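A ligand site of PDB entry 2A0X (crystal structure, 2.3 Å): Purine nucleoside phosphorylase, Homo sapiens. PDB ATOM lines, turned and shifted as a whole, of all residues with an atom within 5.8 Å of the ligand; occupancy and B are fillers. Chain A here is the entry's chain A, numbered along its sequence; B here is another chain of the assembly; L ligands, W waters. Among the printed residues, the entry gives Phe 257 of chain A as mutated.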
ATOM      1  N   SER A  33      24.888  22.293  13.016  1.00  0.00           N
ATOM      2  CA  SER A  33      24.891  23.181  11.854  1.00  0.00           C
ATOM      3  C   SER A  33      23.640  24.061  11.800  1.00  0.00           C
ATOM      4  O   SER A  33      22.514  23.565  11.886  1.00  0.00           O
ATOM      5  CB  SER A  33      24.988  22.364  10.578  1.00  0.00           C
ATOM      6  OG  SER A  33      24.878  23.203   9.438  1.00  0.00           O
ATOM      7  N   HIS A  86      34.301  17.433  12.916  1.00  0.00           N
ATOM      8  CA  HIS A  86      33.744  16.229  12.321  1.00  0.00           C
ATOM      9  C   HIS A  86      34.823  15.288  11.851  1.00  0.00           C
ATOM     10  O   HIS A  86      35.908  15.708  11.443  1.00  0.00           O
ATOM     11  CB  HIS A  86      32.854  16.550  11.113  1.00  0.00           C
ATOM     12  CG  HIS A  86      31.763  17.532  11.395  1.00  0.00           C
ATOM     13  ND1 HIS A  86      31.976  18.896  11.419  1.00  0.00           N
ATOM     14  CD2 HIS A  86      30.443  17.352  11.638  1.00  0.00           C
ATOM     15  CE1 HIS A  86      30.823  19.507  11.649  1.00  0.00           C
ATOM     16  NE2 HIS A  86      29.882  18.598  11.785  1.00  0.00           N
ATOM     17  N   TYR A  88      34.737  13.517   9.156  1.00  0.00           N
ATOM     18  CA  TYR A  88      34.964  13.692   7.723  1.00  0.00           C
ATOM     19  C   TYR A  88      35.963  14.793   7.367  1.00  0.00           C
ATOM     20  O   TYR A  88      36.504  14.794   6.265  1.00  0.00           O
ATOM     21  CB  TYR A  88      33.629  13.928   6.967  1.00  0.00           C
ATOM     22  CG  TYR A  88      32.862  15.185   7.347  1.00  0.00           C
ATOM     23  CD1 TYR A  88      33.375  16.459   7.047  1.00  0.00           C
ATOM     24  CD2 TYR A  88      31.629  15.110   7.997  1.00  0.00           C
ATOM     25  CE1 TYR A  88      32.662  17.617   7.396  1.00  0.00           C
ATOM     26  CE2 TYR A  88      30.912  16.252   8.338  1.00  0.00           C
ATOM     27  CZ  TYR A  88      31.435  17.499   8.046  1.00  0.00           C
ATOM     28  OH  TYR A  88      30.737  18.614   8.417  1.00  0.00           O
ATOM     29  N   ALA A 116      21.996  18.811  12.854  1.00  0.00           N
ATOM     30  CA  ALA A 116      21.047  18.807  11.749  1.00  0.00           C
ATOM     31  C   ALA A 116      21.091  17.344  11.303  1.00  0.00           C
ATOM     32  O   ALA A 116      22.112  16.682  11.498  1.00  0.00           O
ATOM     33  CB  ALA A 116      21.522  19.721  10.630  1.00  0.00           C
ATOM     34  N   ALA A 117      20.014  16.832  10.726  1.00  0.00           N
ATOM     35  CA  ALA A 117      20.011  15.455  10.294  1.00  0.00           C
ATOM     36  C   ALA A 117      18.980  15.193   9.212  1.00  0.00           C
ATOM     37  O   ALA A 117      18.002  15.923   9.082  1.00  0.00           O
ATOM     38  CB  ALA A 117      19.741  14.528  11.482  1.00  0.00           C
ATOM     39  N   GLY A 118      19.228  14.146   8.438  1.00  0.00           N
ATOM     40  CA  GLY A 118      18.321  13.761   7.384  1.00  0.00           C
ATOM     41  C   GLY A 118      17.309  12.849   8.028  1.00  0.00           C
ATOM     42  O   GLY A 118      17.657  12.014   8.864  1.00  0.00           O
ATOM     43  N   GLY A 119      16.051  13.011   7.644  1.00  0.00           N
ATOM     44  CA  GLY A 119      15.013  12.178   8.214  1.00  0.00           C
ATOM     45  C   GLY A 119      14.896  10.877   7.466  1.00  0.00           C
ATOM     46  O   GLY A 119      14.763  10.855   6.254  1.00  0.00           O
ATOM     47  N   VAL A 195      26.933   8.234  10.432  1.00  0.00           N
ATOM     48  CA  VAL A 195      27.707   7.720   9.306  1.00  0.00           C
ATOM     49  C   VAL A 195      28.800   8.761   9.156  1.00  0.00           C
ATOM     50  O   VAL A 195      28.588   9.939   9.492  1.00  0.00           O
ATOM     51  CB  VAL A 195      26.901   7.618   7.978  1.00  0.00           C
ATOM     52  CG1 VAL A 195      25.777   6.598   8.128  1.00  0.00           C
ATOM     53  CG2 VAL A 195      26.377   8.991   7.553  1.00  0.00           C
ATOM     54  N   PHE A 200      26.655  12.463   0.735  1.00  0.00           N
ATOM     55  CA  PHE A 200      25.323  12.059   1.181  1.00  0.00           C
ATOM     56  C   PHE A 200      25.006  10.630   0.759  1.00  0.00           C
ATOM     57  O   PHE A 200      25.590  10.095  -0.186  1.00  0.00           O
ATOM     58  CB  PHE A 200      24.261  13.019   0.653  1.00  0.00           C
ATOM     59  CG  PHE A 200      24.248  14.356   1.350  1.00  0.00           C
ATOM     60  CD1 PHE A 200      24.002  14.431   2.714  1.00  0.00           C
ATOM     61  CD2 PHE A 200      24.466  15.532   0.638  1.00  0.00           C
ATOM     62  CE1 PHE A 200      23.969  15.663   3.380  1.00  0.00           C
ATOM     63  CE2 PHE A 200      24.442  16.772   1.282  1.00  0.00           C
ATOM     64  CZ  PHE A 200      24.188  16.837   2.658  1.00  0.00           C
ATOM     65  N   GLU A 201      24.036  10.034   1.444  1.00  0.00           N
ATOM     66  CA  GLU A 201      23.615   8.663   1.209  1.00  0.00           C
ATOM     67  C   GLU A 201      22.941   8.397  -0.133  1.00  0.00           C
ATOM     68  O   GLU A 201      22.295   9.274  -0.696  1.00  0.00           O
ATOM     69  CB  GLU A 201      22.654   8.202   2.312  1.00  0.00           C
ATOM     70  CG  GLU A 201      23.150   8.327   3.749  1.00  0.00           C
ATOM     71  CD  GLU A 201      23.397   9.767   4.188  1.00  0.00           C
ATOM     72  OE1 GLU A 201      22.614  10.652   3.796  1.00  0.00           O
ATOM     73  OE2 GLU A 201      24.358   9.997   4.943  1.00  0.00           O
ATOM     74  N   VAL A 217      19.650  10.545  10.358  1.00  0.00           N
ATOM     75  CA  VAL A 217      21.042  10.268  10.042  1.00  0.00           C
ATOM     76  C   VAL A 217      21.888  11.548  10.015  1.00  0.00           C
ATOM     77  O   VAL A 217      21.479  12.560   9.452  1.00  0.00           O
ATOM     78  CB  VAL A 217      21.177   9.561   8.675  1.00  0.00           C
ATOM     79  CG1 VAL A 217      20.563  10.433   7.589  1.00  0.00           C
ATOM     80  CG2 VAL A 217      22.629   9.268   8.384  1.00  0.00           C
ATOM     81  N   GLY A 218      23.064  11.465  10.627  1.00  0.00           N
ATOM     82  CA  GLY A 218      23.962  12.605  10.661  1.00  0.00           C
ATOM     83  C   GLY A 218      25.401  12.129  10.636  1.00  0.00           C
ATOM     84  O   GLY A 218      25.678  10.929  10.566  1.00  0.00           O
ATOM     85  N   MET A 219      26.332  13.075  10.719  1.00  0.00           N
ATOM     86  CA  MET A 219      27.741  12.733  10.659  1.00  0.00           C
ATOM     87  C   MET A 219      28.511  13.182  11.894  1.00  0.00           C
ATOM     88  O   MET A 219      29.711  13.441  11.811  1.00  0.00           O
ATOM     89  CB  MET A 219      28.357  13.377   9.416  1.00  0.00           C
ATOM     90  CG  MET A 219      27.610  13.043   8.129  1.00  0.00           C
ATOM     91  SD  MET A 219      28.267  13.941   6.711  1.00  0.00           S
ATOM     92  CE  MET A 219      27.126  13.451   5.444  1.00  0.00           C
ATOM     93  N   THR A 242      16.487  18.534   8.692  1.00  0.00           N
ATOM     94  CA  THR A 242      16.626  19.541   7.651  1.00  0.00           C
ATOM     95  C   THR A 242      16.211  19.044   6.279  1.00  0.00           C
ATOM     96  O   THR A 242      16.088  19.825   5.338  1.00  0.00           O
ATOM     97  CB  THR A 242      18.080  20.028   7.561  1.00  0.00           C
ATOM     98  OG1 THR A 242      18.942  18.912   7.311  1.00  0.00           O
ATOM     99  CG2 THR A 242      18.499  20.716   8.859  1.00  0.00           C
ATOM    100  N   ASN A 243      15.981  17.743   6.145  1.00  0.00           N
ATOM    101  CA  ASN A 243      15.606  17.185   4.856  1.00  0.00           C
ATOM    102  C   ASN A 243      15.157  15.732   4.988  1.00  0.00           C
ATOM    103  O   ASN A 243      15.477  15.071   5.968  1.00  0.00           O
ATOM    104  CB  ASN A 243      16.801  17.255   3.890  1.00  0.00           C
ATOM    105  CG  ASN A 243      18.052  16.567   4.462  1.00  0.00           C
ATOM    106  OD1 ASN A 243      18.609  16.995   5.479  1.00  0.00           O
ATOM    107  ND2 ASN A 243      18.485  15.493   3.808  1.00  0.00           N
ATOM    108  N   VAL A 245      15.609  12.192   3.484  1.00  0.00           N
ATOM    109  CA  VAL A 245      16.524  11.434   2.634  1.00  0.00           C
ATOM    110  C   VAL A 245      15.759  10.706   1.545  1.00  0.00           C
ATOM    111  O   VAL A 245      14.703  10.140   1.793  1.00  0.00           O
ATOM    112  CB  VAL A 245      17.346  10.416   3.477  1.00  0.00           C
ATOM    113  CG1 VAL A 245      18.112  11.144   4.566  1.00  0.00           C
ATOM    114  CG2 VAL A 245      16.424   9.396   4.087  1.00  0.00           C
ATOM    115  N   ALA A 255      19.798  15.669  -1.927  1.00  0.00           N
ATOM    116  CA  ALA A 255      20.230  16.369  -0.721  1.00  0.00           C
ATOM    117  C   ALA A 255      21.398  17.309  -1.013  1.00  0.00           C
ATOM    118  O   ALA A 255      22.298  16.975  -1.794  1.00  0.00           O
ATOM    119  CB  ALA A 255      20.631  15.358   0.360  1.00  0.00           C
ATOM    120  N   ASN A 256      21.379  18.488  -0.395  1.00  0.00           N
ATOM    121  CA  ASN A 256      22.434  19.476  -0.602  1.00  0.00           C
ATOM    122  C   ASN A 256      22.640  20.416   0.584  1.00  0.00           C
ATOM    123  O   ASN A 256      21.739  20.614   1.394  1.00  0.00           O
ATOM    124  CB  ASN A 256      22.143  20.283  -1.880  1.00  0.00           C
ATOM    125  CG  ASN A 256      20.715  20.823  -1.919  1.00  0.00           C
ATOM    126  OD1 ASN A 256      20.319  21.605  -1.059  1.00  0.00           O
ATOM    127  ND2 ASN A 256      19.953  20.389  -2.917  1.00  0.00           N
ATOM    128  N   PHE A 257      23.839  20.996   0.658  1.00  0.00           N
ATOM    129  CA  PHE A 257      24.209  21.929   1.717  1.00  0.00           C
ATOM    130  C   PHE A 257      23.204  23.072   1.865  1.00  0.00           C
ATOM    131  O   PHE A 257      23.007  23.610   2.958  1.00  0.00           O
ATOM    132  CB  PHE A 257      25.601  22.507   1.409  1.00  0.00           C
ATOM    133  CG  PHE A 257      26.132  23.417   2.481  1.00  0.00           C
ATOM    134  CD1 PHE A 257      26.506  22.919   3.724  1.00  0.00           C
ATOM    135  CD2 PHE A 257      26.277  24.787   2.232  1.00  0.00           C
ATOM    136  CE1 PHE A 257      27.034  23.771   4.714  1.00  0.00           C
ATOM    137  CE2 PHE A 257      26.803  25.646   3.210  1.00  0.00           C
ATOM    138  CZ  PHE A 257      27.186  25.128   4.449  1.00  0.00           C
ATOM    139  N   VAL A 260      19.941  21.912   3.917  1.00  0.00           N
ATOM    140  CA  VAL A 260      20.265  21.903   5.344  1.00  0.00           C
ATOM    141  C   VAL A 260      20.263  23.265   6.038  1.00  0.00           C
ATOM    142  O   VAL A 260      19.507  23.479   6.983  1.00  0.00           O
ATOM    143  CB  VAL A 260      21.630  21.211   5.593  1.00  0.00           C
ATOM    144  CG1 VAL A 260      21.903  21.125   7.092  1.00  0.00           C
ATOM    145  CG2 VAL A 260      21.624  19.824   4.977  1.00  0.00           C
ATOM    146  N   LEU A 261      21.117  24.183   5.584  1.00  0.00           N
ATOM    147  CA  LEU A 261      21.180  25.507   6.214  1.00  0.00           C
ATOM    148  C   LEU A 261      19.891  26.308   6.088  1.00  0.00           C
ATOM    149  O   LEU A 261      19.593  27.140   6.953  1.00  0.00           O
ATOM    150  CB  LEU A 261      22.365  26.321   5.653  1.00  0.00           C
ATOM    151  CG  LEU A 261      23.777  25.927   6.104  1.00  0.00           C
ATOM    152  CD1 LEU A 261      24.735  27.052   5.735  1.00  0.00           C
ATOM    153  CD2 LEU A 261      23.809  25.686   7.616  1.00  0.00           C
ATOM    154  N   PHE B 159      29.938  18.450   0.490  1.00  0.00           N
ATOM    155  CA  PHE B 159      28.925  17.416   0.673  1.00  0.00           C
ATOM    156  C   PHE B 159      28.218  17.014  -0.635  1.00  0.00           C
ATOM    157  O   PHE B 159      27.060  17.346  -0.831  1.00  0.00           O
ATOM    158  CB  PHE B 159      27.868  17.908   1.672  1.00  0.00           C
ATOM    159  CG  PHE B 159      28.441  18.430   2.961  1.00  0.00           C
ATOM    160  CD1 PHE B 159      29.051  17.574   3.877  1.00  0.00           C
ATOM    161  CD2 PHE B 159      28.375  19.788   3.261  1.00  0.00           C
ATOM    162  CE1 PHE B 159      29.593  18.059   5.076  1.00  0.00           C
ATOM    163  CE2 PHE B 159      28.910  20.291   4.455  1.00  0.00           C
ATOM    164  CZ  PHE B 159      29.525  19.424   5.364  1.00  0.00           C
HETATM  165  O1  LIG L   1      24.668  19.811   5.006  1.00  0.00           O
HETATM  166  C1  LIG L   1      25.554  18.915   5.646  1.00  0.00           C
HETATM  167  C2  LIG L   1      25.863  18.806   7.093  1.00  0.00           C
HETATM  168  C3  LIG L   1      24.620  18.498   7.834  1.00  0.00           C
HETATM  169  C4  LIG L   1      26.847  17.731   7.405  1.00  0.00           C
HETATM  170  O2  LIG L   1      27.888  18.052   8.330  1.00  0.00           O
HETATM  171  C5  LIG L   1      25.848  16.690   7.737  1.00  0.00           C
HETATM  172  N1  LIG L   1      24.847  17.283   8.588  1.00  0.00           N
HETATM  173  C6  LIG L   1      23.623  16.532   8.766  1.00  0.00           C
HETATM  174  C7  LIG L   1      22.678  16.050   7.727  1.00  0.00           C
HETATM  175  C8  LIG L   1      21.560  16.668   7.203  1.00  0.00           C
HETATM  176  N2  LIG L   1      20.935  15.988   6.283  1.00  0.00           N
HETATM  177  C9  LIG L   1      21.658  14.818   6.146  1.00  0.00           C
HETATM  178  C10 LIG L   1      21.447  13.672   5.254  1.00  0.00           C
HETATM  179  O3  LIG L   1      20.549  13.537   4.436  1.00  0.00           O
HETATM  180  N3  LIG L   1      22.419  12.633   5.400  1.00  0.00           N
HETATM  181  C11 LIG L   1      23.506  12.682   6.320  1.00  0.00           C
HETATM  182  N4  LIG L   1      23.706  13.762   7.153  1.00  0.00           N
HETATM  183  C12 LIG L   1      22.749  14.812   7.027  1.00  0.00           C
HETATM  184  O   HOH W   1      20.775  11.970   2.227  1.00  0.00           O
HETATM  185  O   HOH W   2      26.917  16.163  10.734  1.00  0.00           O
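OD1 of Asn 243 sits at hydrogen-bond distance from OG1 of Thr 242 (2.7 Å). The backbone carbonyl oxygen (O) of Asn 243 sits at hydrogen-bond distance from the backbone NH (N) of Gly 119 (2.7 Å). A ring nitrogen (ND1) of His 86 is in hydrogen-bond range of the side-chain hydroxyl (OH) of Tyr 88 (3.3 Å). The backbone carbonyl oxygen of Gly 118 is in hydrogen-bond range of the backbone NH of Val 217 (2.9 Å). The backbone NH (N) of Val 245 sits close to the backbone carbonyl oxygen (O) of Gly 119, 3.2 Å away. The backbone NH of Thr 242 lies within hydrogen-bond range of the backbone carbonyl oxygen of Ala 117 (3.0 Å). The backbone carbonyl oxygen (O) of Gly 218 sits at hydrogen-bond distance from the backbone NH (N) of Val 195 (3.0 Å).
O of Ala 116 touches C6 of the ligand (3.1 Å). Ala 117 touches the ligand (C to C8, 3.6 Å). Phe 200 touches the ligand (CD1 to N3, 3.6 Å). CA of Gly 218 touches N4 of the ligand (3.7 Å). Met 219 touches the ligand. Thr 242 touches the ligand. Val 245 touches the ligand (CG1 to O3, 3.4 Å). Phe 257 touches the ligand (CD1 to O1, 3.8 Å). CG2 of Val 260 touches O1 of the ligand (3.0 Å). CE1 of Phe 159 of chain B touches C4 of the ligand, 3.6 Å away. 15 residues have an atom within 4 Å of the ligand: Tyr 88, Ala 116, Ala 117, Gly 118, Phe 200, Glu 201, Val 217, Gly 218, Met 219, Thr 242, Asn 243, Val 245, Phe 257, Val 260 and Phe 159 of chain B.
The side-chain carboxylate (OE1) of Glu 201 is in hydrogen-bond range of a nitrogen (N3) of the ligand (2.6 Å). The side-chain amide oxygen of Asn 243 sits at hydrogen-bond distance from a nitrogen (N2) of the ligand. An oxygen (O2) of the ligand sits at hydrogen-bond distance from the side-chain hydroxyl of Tyr 88 (2.9 Å). N of Gly 118 sits close to N2 of the ligand, at 3.3 Å. O of Val 217 lies close to N4 of the ligand (3.4 Å).
Water W1 bridges an oxygen (O3) of the ligand and the side-chain carboxylate of Glu 201. Water W2 lies within hydrogen-bond range of N of Met 219 and N1 of the ligand.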
